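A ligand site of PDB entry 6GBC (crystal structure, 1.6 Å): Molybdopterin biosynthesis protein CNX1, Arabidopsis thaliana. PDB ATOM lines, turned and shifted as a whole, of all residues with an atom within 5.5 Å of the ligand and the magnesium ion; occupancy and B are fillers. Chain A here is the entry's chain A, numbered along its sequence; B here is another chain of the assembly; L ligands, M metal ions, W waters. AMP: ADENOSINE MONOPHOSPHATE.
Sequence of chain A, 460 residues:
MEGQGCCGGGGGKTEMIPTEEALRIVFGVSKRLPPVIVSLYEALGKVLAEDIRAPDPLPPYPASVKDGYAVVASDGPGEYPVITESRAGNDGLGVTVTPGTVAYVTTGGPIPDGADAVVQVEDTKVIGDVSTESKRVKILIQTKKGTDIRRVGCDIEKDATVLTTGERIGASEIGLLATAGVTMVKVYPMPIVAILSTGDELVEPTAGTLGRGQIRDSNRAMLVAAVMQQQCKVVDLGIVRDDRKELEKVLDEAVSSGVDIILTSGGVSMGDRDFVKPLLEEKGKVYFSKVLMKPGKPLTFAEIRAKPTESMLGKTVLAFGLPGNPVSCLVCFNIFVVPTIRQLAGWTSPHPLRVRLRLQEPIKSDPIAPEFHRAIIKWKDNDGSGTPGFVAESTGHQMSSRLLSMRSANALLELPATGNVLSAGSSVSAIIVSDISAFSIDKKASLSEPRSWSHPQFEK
Merely in contact with the magnesium ion: Glu 201 and Gly 267.
Of the 28 residues printed, 2 come within 4 Å of the magnesium ion.
An oxygen (O4') of the ligand sits close to the backbone carbonyl oxygen (O) of Gly 324, 3.0 Å away.
Merely in contact with the ligand: Thr 198 (3.8 Å), Leu 202 (3.7 Å), Ile 215 (3.6 Å), Ser 265 (3.99 Å), Gly 266 (3.4 Å), Val 268 (3.998 Å), Pro 326 (3.9 Å), Thr 107 of chain B (3.5 Å), Gly 108 of chain B (3.4 Å) and Arg 150 of chain B (3.7 Å).
19 residues have an atom within 4 Å of the ligand: Ser 197, Thr 198, Glu 201, Leu 202, Ile 215, Asp 217, Ser 218, Asn 219, Ser 265, Gly 266, Gly 267, Val 268, Ser 269, Gly 324, Asn 325, Pro 326, Thr 107 of chain B, Gly 108 of chain B and Arg 150 of chain B.
The nearest printed residue that does not touch the ligand is Arg 216 (4.004 Å).
The side-chain carboxylate (OE2) of Glu 201 sits at hydrogen-bond distance from an oxygen (O2') of the ligand (2.7 Å).
OD1 of Asp 217 is in hydrogen-bond range of N6 of the ligand (2.8 Å).
An oxygen (O3P) of the ligand is in hydrogen-bond range of the backbone NH (N) of Gly 267.
An oxygen (O3P) of the ligand lies within hydrogen-bond range of the side-chain hydroxyl of Ser 269 (3.0 Å).
The backbone NH (N) of Asn 325 sits at hydrogen-bond distance from an oxygen (O4') of the ligand (3.1 Å).
N1 of the ligand is in hydrogen-bond range of N of Ser 218, at 3.2 Å.
N1 of the ligand lies close to OG of Ser 218 (3.5 Å).
N6 of the ligand is in hydrogen-bond range of OG of Ser 197, 3.2 Å away.
N of Asn 219 sits at hydrogen-bond distance from N1 of the ligand (3.3 Å).
Water W12 bridges OE1 of Glu 201 and OD2 of Asp 242.
Water W5 lies within hydrogen-bond range of OD1 of Asp 242 (2.9 Å), OG1 of Thr 198 (2.9 Å) and N of Gly 267 (3.1 Å).
Water W7 lies within hydrogen-bond range of OD2 of Asp 274 (2.6 Å), O1P of the ligand (2.6 Å) and OD1 of Asp 67 of chain B (2.7 Å).
Water W10 lies within hydrogen-bond range of an oxygen (O3') of the ligand (2.7 Å), the backbone carbonyl oxygen of Ser 64 of chain B (2.8 Å), the guanidinium group of Arg 150 of chain B (3.0 Å) and the backbone NH of Gly 108 of chain B (3.5 Å).
Water W6 lies within hydrogen-bond range of the side-chain amide oxygen of Asn 325 (2.7 Å), an oxygen (O3') of the ligand (2.8 Å) and the guanidinium group of Arg 150 of chain B (3.4 Å).
Water W4 lies within hydrogen-bond range of an oxygen (O2') of the ligand, the side-chain hydroxyl of Tyr 61 of chain B and the guanidinium group of Arg 150 of chain B.
The side-chain carboxylate (OD1) of Asp 217 lies within hydrogen-bond range of the side-chain hydroxyl (OG) of Ser 197 (2.7 Å).
OD2 of Asp 217 is in salt-bridge range of NE of Arg 220 (2.8 Å).
The backbone NH (N) of Gly 267 sits at hydrogen-bond distance from the side-chain hydroxyl (OG1) of Thr 198 (3.3 Å).
The backbone carbonyl oxygen of Gly 324 sits at hydrogen-bond distance from the side-chain amide nitrogen of Asn 219, at 2.8 Å.
N of Ser 269 lies within hydrogen-bond range of OD2 of Asp 274.
O of Gly 108 of chain B lies within hydrogen-bond range of OH of Tyr 61 of chain B, 2.7 Å away.
O of Ser 64 of chain B is in hydrogen-bond range of N of Gly 108 of chain B (2.8 Å).
N of Thr 107 of chain B sits at hydrogen-bond distance from OD1 of Asp 67 of chain B.
The magnesium ion is bound by an oxygen (O2P) of the ligand (2.0 Å), water W5 (2.0 Å), water W11 (2.1 Å), water W1 (2.1 Å), water W3 (2.1 Å) and water W12 (2.1 Å).
The magnesium ion has six donor atoms within binding distance.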
ATOM      1  N   SER A 197     -12.875  14.592 -13.605  1.00  0.00           N
ATOM      2  CA  SER A 197     -11.446  14.268 -13.468  1.00  0.00           C
ATOM      3  C   SER A 197     -11.007  13.622 -14.743  1.00  0.00           C
ATOM      4  O   SER A 197     -11.817  13.008 -15.445  1.00  0.00           O
ATOM      5  CB  SER A 197     -11.212  13.307 -12.297  1.00  0.00           C
ATOM      6  OG  SER A 197     -11.257  14.007 -11.058  1.00  0.00           O
ATOM      7  N   THR A 198      -9.696  13.691 -15.044  1.00  0.00           N
ATOM      8  CA  THR A 198      -9.193  13.032 -16.252  1.00  0.00           C
ATOM      9  C   THR A 198      -8.043  12.117 -15.899  1.00  0.00           C
ATOM     10  O   THR A 198      -7.207  12.466 -15.059  1.00  0.00           O
ATOM     11  CB  THR A 198      -8.749  14.044 -17.315  1.00  0.00           C
ATOM     12  OG1 THR A 198      -7.559  14.710 -16.911  1.00  0.00           O
ATOM     13  CG2 THR A 198      -9.830  15.059 -17.672  1.00  0.00           C
ATOM     14  N   GLY A 199      -7.965  10.982 -16.573  1.00  0.00           N
ATOM     15  CA  GLY A 199      -6.794  10.133 -16.406  1.00  0.00           C
ATOM     16  C   GLY A 199      -7.041   8.653 -16.523  1.00  0.00           C
ATOM     17  O   GLY A 199      -7.898   8.110 -15.839  1.00  0.00           O
ATOM     18  N   GLU A 201      -4.989   6.587 -15.307  1.00  0.00           N
ATOM     19  CA  GLU A 201      -4.463   6.040 -14.060  1.00  0.00           C
ATOM     20  C   GLU A 201      -5.482   6.094 -12.928  1.00  0.00           C
ATOM     21  O   GLU A 201      -5.247   5.507 -11.888  1.00  0.00           O
ATOM     22  CB  GLU A 201      -3.124   6.740 -13.653  1.00  0.00           C
ATOM     23  CG  GLU A 201      -3.169   8.133 -13.020  1.00  0.00           C
ATOM     24  CD  GLU A 201      -3.533   9.302 -13.900  1.00  0.00           C
ATOM     25  OE1 GLU A 201      -4.011   9.063 -15.033  1.00  0.00           O
ATOM     26  OE2 GLU A 201      -3.318  10.461 -13.483  1.00  0.00           O
ATOM     27  N   LEU A 202      -6.594   6.851 -13.088  1.00  0.00           N
ATOM     28  CA  LEU A 202      -7.526   7.027 -11.984  1.00  0.00           C
ATOM     29  C   LEU A 202      -8.443   5.881 -11.785  1.00  0.00           C
ATOM     30  O   LEU A 202      -8.933   5.297 -12.756  1.00  0.00           O
ATOM     31  CB  LEU A 202      -8.376   8.285 -12.201  1.00  0.00           C
ATOM     32  CG  LEU A 202      -7.615   9.575 -12.445  1.00  0.00           C
ATOM     33  CD1 LEU A 202      -8.585  10.721 -12.672  1.00  0.00           C
ATOM     34  CD2 LEU A 202      -6.659   9.885 -11.287  1.00  0.00           C
ATOM     35  N   ILE A 215      -4.166   5.122  -9.138  1.00  0.00           N
ATOM     36  CA  ILE A 215      -4.336   5.934  -7.919  1.00  0.00           C
ATOM     37  C   ILE A 215      -5.816   6.239  -7.800  1.00  0.00           C
ATOM     38  O   ILE A 215      -6.516   6.324  -8.820  1.00  0.00           O
ATOM     39  CB  ILE A 215      -3.550   7.268  -7.983  1.00  0.00           C
ATOM     40  CG1 ILE A 215      -3.946   8.124  -9.214  1.00  0.00           C
ATOM     41  CG2 ILE A 215      -2.060   6.979  -7.998  1.00  0.00           C
ATOM     42  CD1 ILE A 215      -3.454   9.567  -9.149  1.00  0.00           C
ATOM     43  N   ARG A 216      -6.284   6.546  -6.595  1.00  0.00           N
ATOM     44  CA  ARG A 216      -7.692   6.953  -6.455  1.00  0.00           C
ATOM     45  C   ARG A 216      -7.877   8.382  -6.940  1.00  0.00           C
ATOM     46  O   ARG A 216      -7.009   9.246  -6.717  1.00  0.00           O
ATOM     47  CB  ARG A 216      -8.153   6.822  -4.983  1.00  0.00           C
ATOM     48  CG  ARG A 216      -8.120   5.376  -4.527  1.00  0.00           C
ATOM     49  CD  ARG A 216      -8.686   5.164  -3.129  1.00  0.00           C
ATOM     50  NE  ARG A 216      -8.382   3.780  -2.725  1.00  0.00           N
ATOM     51  CZ  ARG A 216      -7.237   3.370  -2.191  1.00  0.00           C
ATOM     52  NH1 ARG A 216      -6.282   4.252  -1.884  1.00  0.00           N
ATOM     53  NH2 ARG A 216      -7.030   2.080  -1.943  1.00  0.00           N
ATOM     54  N   ASP A 217      -8.992   8.647  -7.617  1.00  0.00           N
ATOM     55  CA  ASP A 217      -9.344  10.001  -8.010  1.00  0.00           C
ATOM     56  C   ASP A 217      -9.647  10.797  -6.703  1.00  0.00           C
ATOM     57  O   ASP A 217     -10.643  10.517  -6.014  1.00  0.00           O
ATOM     58  CB  ASP A 217     -10.619   9.948  -8.848  1.00  0.00           C
ATOM     59  CG  ASP A 217     -11.217  11.248  -9.295  1.00  0.00           C
ATOM     60  OD1 ASP A 217     -10.594  12.303  -9.064  1.00  0.00           O
ATOM     61  OD2 ASP A 217     -12.311  11.216  -9.889  1.00  0.00           O
ATOM     62  N   SER A 218      -8.756  11.716  -6.317  1.00  0.00           N
ATOM     63  CA  SER A 218      -8.979  12.537  -5.123  1.00  0.00           C
ATOM     64  C   SER A 218      -9.419  13.970  -5.527  1.00  0.00           C
ATOM     65  O   SER A 218     -10.103  14.621  -4.757  1.00  0.00           O
ATOM     66  CB  SER A 218      -7.728  12.597  -4.242  1.00  0.00           C
ATOM     67  OG  SER A 218      -6.647  13.191  -4.945  1.00  0.00           O
ATOM     68  N   ASN A 219      -9.005  14.467  -6.702  1.00  0.00           N
ATOM     69  CA  ASN A 219      -9.355  15.857  -7.072  1.00  0.00           C
ATOM     70  C   ASN A 219     -10.837  16.076  -7.199  1.00  0.00           C
ATOM     71  O   ASN A 219     -11.320  17.161  -6.866  1.00  0.00           O
ATOM     72  CB  ASN A 219      -8.722  16.259  -8.417  1.00  0.00           C
ATOM     73  CG  ASN A 219      -7.235  16.435  -8.372  1.00  0.00           C
ATOM     74  OD1 ASN A 219      -6.631  16.460  -7.306  1.00  0.00           O
ATOM     75  ND2 ASN A 219      -6.613  16.562  -9.533  1.00  0.00           N
ATOM     76  N   ARG A 220     -11.545  15.096  -7.741  1.00  0.00           N
ATOM     77  CA  ARG A 220     -12.968  15.299  -7.980  1.00  0.00           C
ATOM     78  C   ARG A 220     -13.702  15.488  -6.687  1.00  0.00           C
ATOM     79  O   ARG A 220     -14.396  16.496  -6.546  1.00  0.00           O
ATOM     80  CB  ARG A 220     -13.566  14.147  -8.800  1.00  0.00           C
ATOM     81  CG  ARG A 220     -15.066  14.354  -9.158  1.00  0.00           C
ATOM     82  CD  ARG A 220     -15.400  13.495 -10.383  1.00  0.00           C
ATOM     83  NE  ARG A 220     -14.898  12.123 -10.185  1.00  0.00           N
ATOM     84  CZ  ARG A 220     -15.557  11.097  -9.666  1.00  0.00           C
ATOM     85  NH1 ARG A 220     -16.878  11.175  -9.436  1.00  0.00           N
ATOM     86  NH2 ARG A 220     -14.939   9.936  -9.479  1.00  0.00           N
ATOM     87  N   ASP A 242      -8.131   9.367 -20.970  1.00  0.00           N
ATOM     88  CA  ASP A 242      -7.242  10.191 -21.837  1.00  0.00           C
ATOM     89  C   ASP A 242      -7.502   9.815 -23.287  1.00  0.00           C
ATOM     90  O   ASP A 242      -6.665   9.207 -23.952  1.00  0.00           O
ATOM     91  CB  ASP A 242      -5.780  10.003 -21.426  1.00  0.00           C
ATOM     92  CG  ASP A 242      -5.542  10.425 -19.980  1.00  0.00           C
ATOM     93  OD1 ASP A 242      -6.102  11.466 -19.571  1.00  0.00           O
ATOM     94  OD2 ASP A 242      -4.820   9.713 -19.268  1.00  0.00           O
ATOM     95  N   SER A 265      -9.804  18.601 -14.114  1.00  0.00           N
ATOM     96  CA  SER A 265      -8.438  18.579 -13.574  1.00  0.00           C
ATOM     97  C   SER A 265      -7.628  17.560 -14.368  1.00  0.00           C
ATOM     98  O   SER A 265      -8.203  16.629 -14.930  1.00  0.00           O
ATOM     99  CB  SER A 265      -8.402  18.328 -12.069  1.00  0.00           C
ATOM    100  OG  SER A 265      -8.593  16.965 -11.701  1.00  0.00           O
ATOM    101  N   GLY A 266      -6.318  17.798 -14.513  1.00  0.00           N
ATOM    102  CA  GLY A 266      -5.422  16.939 -15.275  1.00  0.00           C
ATOM    103  C   GLY A 266      -5.605  17.111 -16.765  1.00  0.00           C
ATOM    104  O   GLY A 266      -6.427  17.921 -17.200  1.00  0.00           O
ATOM    105  N   GLY A 267      -4.845  16.374 -17.576  1.00  0.00           N
ATOM    106  CA  GLY A 267      -4.971  16.457 -19.022  1.00  0.00           C
ATOM    107  C   GLY A 267      -4.582  17.791 -19.611  1.00  0.00           C
ATOM    108  O   GLY A 267      -4.986  18.103 -20.747  1.00  0.00           O
ATOM    109  N   VAL A 268      -3.819  18.610 -18.845  1.00  0.00           N
ATOM    110  CA  VAL A 268      -3.431  19.976 -19.234  1.00  0.00           C
ATOM    111  C   VAL A 268      -1.930  20.188 -19.193  1.00  0.00           C
ATOM    112  O   VAL A 268      -1.528  21.343 -19.289  1.00  0.00           O
ATOM    113  CB  VAL A 268      -4.098  21.090 -18.349  1.00  0.00           C
ATOM    114  CG1 VAL A 268      -5.511  21.392 -18.812  1.00  0.00           C
ATOM    115  CG2 VAL A 268      -4.041  20.758 -16.863  1.00  0.00           C
ATOM    116  N   SER A 269      -1.098  19.145 -19.038  1.00  0.00           N
ATOM    117  CA  SER A 269       0.348  19.379 -18.976  1.00  0.00           C
ATOM    118  C   SER A 269       0.913  19.180 -20.398  1.00  0.00           C
ATOM    119  O   SER A 269       0.261  19.592 -21.370  1.00  0.00           O
ATOM    120  CB  SER A 269       1.021  18.444 -17.959  1.00  0.00           C
ATOM    121  OG  SER A 269       0.417  18.480 -16.673  1.00  0.00           O
ATOM    122  N   ASP A 274      -2.893  14.645 -23.357  1.00  0.00           N
ATOM    123  CA  ASP A 274      -3.492  15.744 -22.573  1.00  0.00           C
ATOM    124  C   ASP A 274      -4.351  16.526 -23.558  1.00  0.00           C
ATOM    125  O   ASP A 274      -3.826  17.256 -24.382  1.00  0.00           O
ATOM    126  CB  ASP A 274      -2.347  16.605 -21.956  1.00  0.00           C
ATOM    127  CG  ASP A 274      -1.701  15.932 -20.744  1.00  0.00           C
ATOM    128  OD1 ASP A 274      -2.204  14.877 -20.309  1.00  0.00           O
ATOM    129  OD2 ASP A 274      -0.692  16.443 -20.251  1.00  0.00           O
ATOM    130  N   PRO A 323      -4.898  22.264 -13.010  1.00  0.00           N
ATOM    131  CA  PRO A 323      -3.795  21.283 -13.039  1.00  0.00           C
ATOM    132  C   PRO A 323      -4.186  19.972 -12.328  1.00  0.00           C
ATOM    133  O   PRO A 323      -5.022  19.984 -11.423  1.00  0.00           O
ATOM    134  CB  PRO A 323      -2.668  21.982 -12.284  1.00  0.00           C
ATOM    135  CG  PRO A 323      -3.031  23.436 -12.291  1.00  0.00           C
ATOM    136  CD  PRO A 323      -4.526  23.492 -12.293  1.00  0.00           C
ATOM    137  N   GLY A 324      -3.578  18.867 -12.759  1.00  0.00           N
ATOM    138  CA  GLY A 324      -3.882  17.547 -12.171  1.00  0.00           C
ATOM    139  C   GLY A 324      -3.263  17.350 -10.796  1.00  0.00           C
ATOM    140  O   GLY A 324      -3.822  16.637  -9.957  1.00  0.00           O
ATOM    141  N   ASN A 325      -2.075  17.922 -10.559  1.00  0.00           N
ATOM    142  CA  ASN A 325      -1.448  17.770  -9.228  1.00  0.00           C
ATOM    143  C   ASN A 325      -2.405  18.234  -8.115  1.00  0.00           C
ATOM    144  O   ASN A 325      -2.914  19.355  -8.221  1.00  0.00           O
ATOM    145  CB  ASN A 325      -0.125  18.510  -9.162  1.00  0.00           C
ATOM    146  CG  ASN A 325       1.001  17.704  -9.761  1.00  0.00           C
ATOM    147  OD1 ASN A 325       1.263  16.538  -9.368  1.00  0.00           O
ATOM    148  ND2 ASN A 325       1.692  18.282 -10.714  1.00  0.00           N
ATOM    149  N   PRO A 326      -2.761  17.370  -7.134  1.00  0.00           N
ATOM    150  CA  PRO A 326      -3.763  17.766  -6.108  1.00  0.00           C
ATOM    151  C   PRO A 326      -3.600  19.153  -5.467  1.00  0.00           C
ATOM    152  O   PRO A 326      -4.564  19.869  -5.374  1.00  0.00           O
ATOM    153  CB  PRO A 326      -3.624  16.669  -5.060  1.00  0.00           C
ATOM    154  CG  PRO A 326      -3.318  15.451  -5.885  1.00  0.00           C
ATOM    155  CD  PRO A 326      -2.336  15.968  -6.923  1.00  0.00           C
ATOM    156  N   TYR B  61       3.313   3.512  -6.899  1.00  0.00           N
ATOM    157  CA  TYR B  61       4.306   3.084  -7.873  1.00  0.00           C
ATOM    158  C   TYR B  61       5.242   4.281  -8.089  1.00  0.00           C
ATOM    159  O   TYR B  61       4.794   5.425  -7.891  1.00  0.00           O
ATOM    160  CB  TYR B  61       3.618   2.686  -9.203  1.00  0.00           C
ATOM    161  CG  TYR B  61       2.741   3.759  -9.773  1.00  0.00           C
ATOM    162  CD1 TYR B  61       1.399   3.872  -9.400  1.00  0.00           C
ATOM    163  CD2 TYR B  61       3.254   4.749 -10.596  1.00  0.00           C
ATOM    164  CE1 TYR B  61       0.595   4.899  -9.889  1.00  0.00           C
ATOM    165  CE2 TYR B  61       2.475   5.808 -11.045  1.00  0.00           C
ATOM    166  CZ  TYR B  61       1.145   5.873 -10.703  1.00  0.00           C
ATOM    167  OH  TYR B  61       0.366   6.902 -11.158  1.00  0.00           O
ATOM    168  N   SER B  64       6.379   9.433 -12.625  1.00  0.00           N
ATOM    169  CA  SER B  64       7.060  10.547 -13.246  1.00  0.00           C
ATOM    170  C   SER B  64       6.434  11.853 -12.814  1.00  0.00           C
ATOM    171  O   SER B  64       5.206  11.965 -12.777  1.00  0.00           O
ATOM    172  CB  SER B  64       7.001  10.438 -14.763  1.00  0.00           C
ATOM    173  OG  SER B  64       7.726  11.516 -15.317  1.00  0.00           O
ATOM    174  N   ASP B  67       6.253  15.095 -18.175  1.00  0.00           N
ATOM    175  CA  ASP B  67       6.035  14.479 -19.473  1.00  0.00           C
ATOM    176  C   ASP B  67       7.411  14.516 -20.100  1.00  0.00           C
ATOM    177  O   ASP B  67       8.060  15.560 -20.106  1.00  0.00           O
ATOM    178  CB  ASP B  67       5.036  15.282 -20.297  1.00  0.00           C
ATOM    179  CG  ASP B  67       3.728  15.421 -19.529  1.00  0.00           C
ATOM    180  OD1 ASP B  67       3.032  14.406 -19.368  1.00  0.00           O
ATOM    181  OD2 ASP B  67       3.447  16.525 -19.030  1.00  0.00           O
ATOM    182  N   THR B 107       3.315  12.691 -17.063  1.00  0.00           N
ATOM    183  CA  THR B 107       3.277  12.990 -15.627  1.00  0.00           C
ATOM    184  C   THR B 107       2.296  12.014 -14.990  1.00  0.00           C
ATOM    185  O   THR B 107       1.199  11.836 -15.511  1.00  0.00           O
ATOM    186  CB  THR B 107       2.827  14.459 -15.387  1.00  0.00           C
ATOM    187  OG1 THR B 107       3.708  15.336 -16.111  1.00  0.00           O
ATOM    188  CG2 THR B 107       2.874  14.843 -13.932  1.00  0.00           C
ATOM    189  N   GLY B 108       2.727  11.359 -13.921  1.00  0.00           N
ATOM    190  CA  GLY B 108       1.937  10.344 -13.236  1.00  0.00           C
ATOM    191  C   GLY B 108       2.108   8.955 -13.821  1.00  0.00           C
ATOM    192  O   GLY B 108       1.611   7.988 -13.247  1.00  0.00           O
ATOM    193  N   ARG B 150       8.782  10.610  -8.460  1.00  0.00           N
ATOM    194  CA  ARG B 150       8.177  10.532  -7.139  1.00  0.00           C
ATOM    195  C   ARG B 150       8.335   9.081  -6.713  1.00  0.00           C
ATOM    196  O   ARG B 150       7.660   8.212  -7.260  1.00  0.00           O
ATOM    197  CB  ARG B 150       6.670  10.880  -7.204  1.00  0.00           C
ATOM    198  CG  ARG B 150       6.442  12.371  -7.346  1.00  0.00           C
ATOM    199  CD  ARG B 150       5.051  12.677  -7.869  1.00  0.00           C
ATOM    200  NE  ARG B 150       4.027  12.182  -6.943  1.00  0.00           N
ATOM    201  CZ  ARG B 150       2.916  11.533  -7.275  1.00  0.00           C
ATOM    202  NH1 ARG B 150       2.623  11.303  -8.543  1.00  0.00           N
ATOM    203  NH2 ARG B 150       2.086  11.090  -6.327  1.00  0.00           N
HETATM  204  P   AMP L   1      -1.874  15.441 -15.613  1.00  0.00           P
HETATM  205  O1P AMP L   1      -0.557  14.937 -16.161  1.00  0.00           O
HETATM  206  O2P AMP L   1      -3.040  14.664 -16.150  1.00  0.00           O
HETATM  207  O3P AMP L   1      -1.997  16.930 -15.708  1.00  0.00           O
HETATM  208  O5' AMP L   1      -1.752  15.108 -14.051  1.00  0.00           O
HETATM  209  C5' AMP L   1      -0.717  15.663 -13.247  1.00  0.00           C
HETATM  210  C4' AMP L   1      -0.500  14.808 -12.018  1.00  0.00           C
HETATM  211  O4' AMP L   1      -1.710  14.875 -11.212  1.00  0.00           O
HETATM  212  C3' AMP L   1      -0.229  13.316 -12.275  1.00  0.00           C
HETATM  213  O3' AMP L   1       0.723  12.866 -11.292  1.00  0.00           O
HETATM  214  C2' AMP L   1      -1.585  12.676 -12.035  1.00  0.00           C
HETATM  215  O2' AMP L   1      -1.511  11.283 -11.717  1.00  0.00           O
HETATM  216  C1' AMP L   1      -2.197  13.570 -10.939  1.00  0.00           C
HETATM  217  N9  AMP L   1      -3.675  13.599 -11.056  1.00  0.00           N
HETATM  218  C8  AMP L   1      -4.394  13.922 -12.148  1.00  0.00           C
HETATM  219  N7  AMP L   1      -5.724  13.880 -11.887  1.00  0.00           N
HETATM  220  C5  AMP L   1      -5.836  13.500 -10.590  1.00  0.00           C
HETATM  221  C6  AMP L   1      -6.964  13.204  -9.680  1.00  0.00           C
HETATM  222  N6  AMP L   1      -8.229  13.321 -10.124  1.00  0.00           N
HETATM  223  N1  AMP L   1      -6.687  12.862  -8.405  1.00  0.00           N
HETATM  224  C2  AMP L   1      -5.414  12.734  -7.957  1.00  0.00           C
HETATM  225  N3  AMP L   1      -4.328  12.983  -8.737  1.00  0.00           N
HETATM  226  C4  AMP L   1      -4.494  13.351 -10.033  1.00  0.00           C
HETATM  227 MG    MG M   1      -3.408  12.777 -16.608  1.00  0.00          MG
HETATM  228  O   HOH W   1      -1.693  12.105 -15.570  1.00  0.00           O
HETATM  229  O   HOH W   2      -8.257  14.547 -12.855  1.00  0.00           O
HETATM  230  O   HOH W   3      -2.385  12.962 -18.459  1.00  0.00           O
HETATM  231  O   HOH W   4       0.262   9.788 -10.019  1.00  0.00           O
HETATM  232  O   HOH W   5      -5.142  13.273 -17.577  1.00  0.00           O
HETATM  233  O   HOH W   6       0.516  14.000  -8.754  1.00  0.00           O
HETATM  234  O   HOH W   7       0.463  14.811 -18.568  1.00  0.00           O
HETATM  235  O   HOH W   8      -2.326  12.162  -6.838  1.00  0.00           O
HETATM  236  O   HOH W   9      -1.523  19.288 -14.771  1.00  0.00           O
HETATM  237  O   HOH W  10       3.411  12.915 -10.886  1.00  0.00           O
HETATM  238  O   HOH W  11      -4.417  12.410 -14.851  1.00  0.00           O
HETATM  239  O   HOH W  12      -3.483  10.689 -17.074  1.00  0.00           O
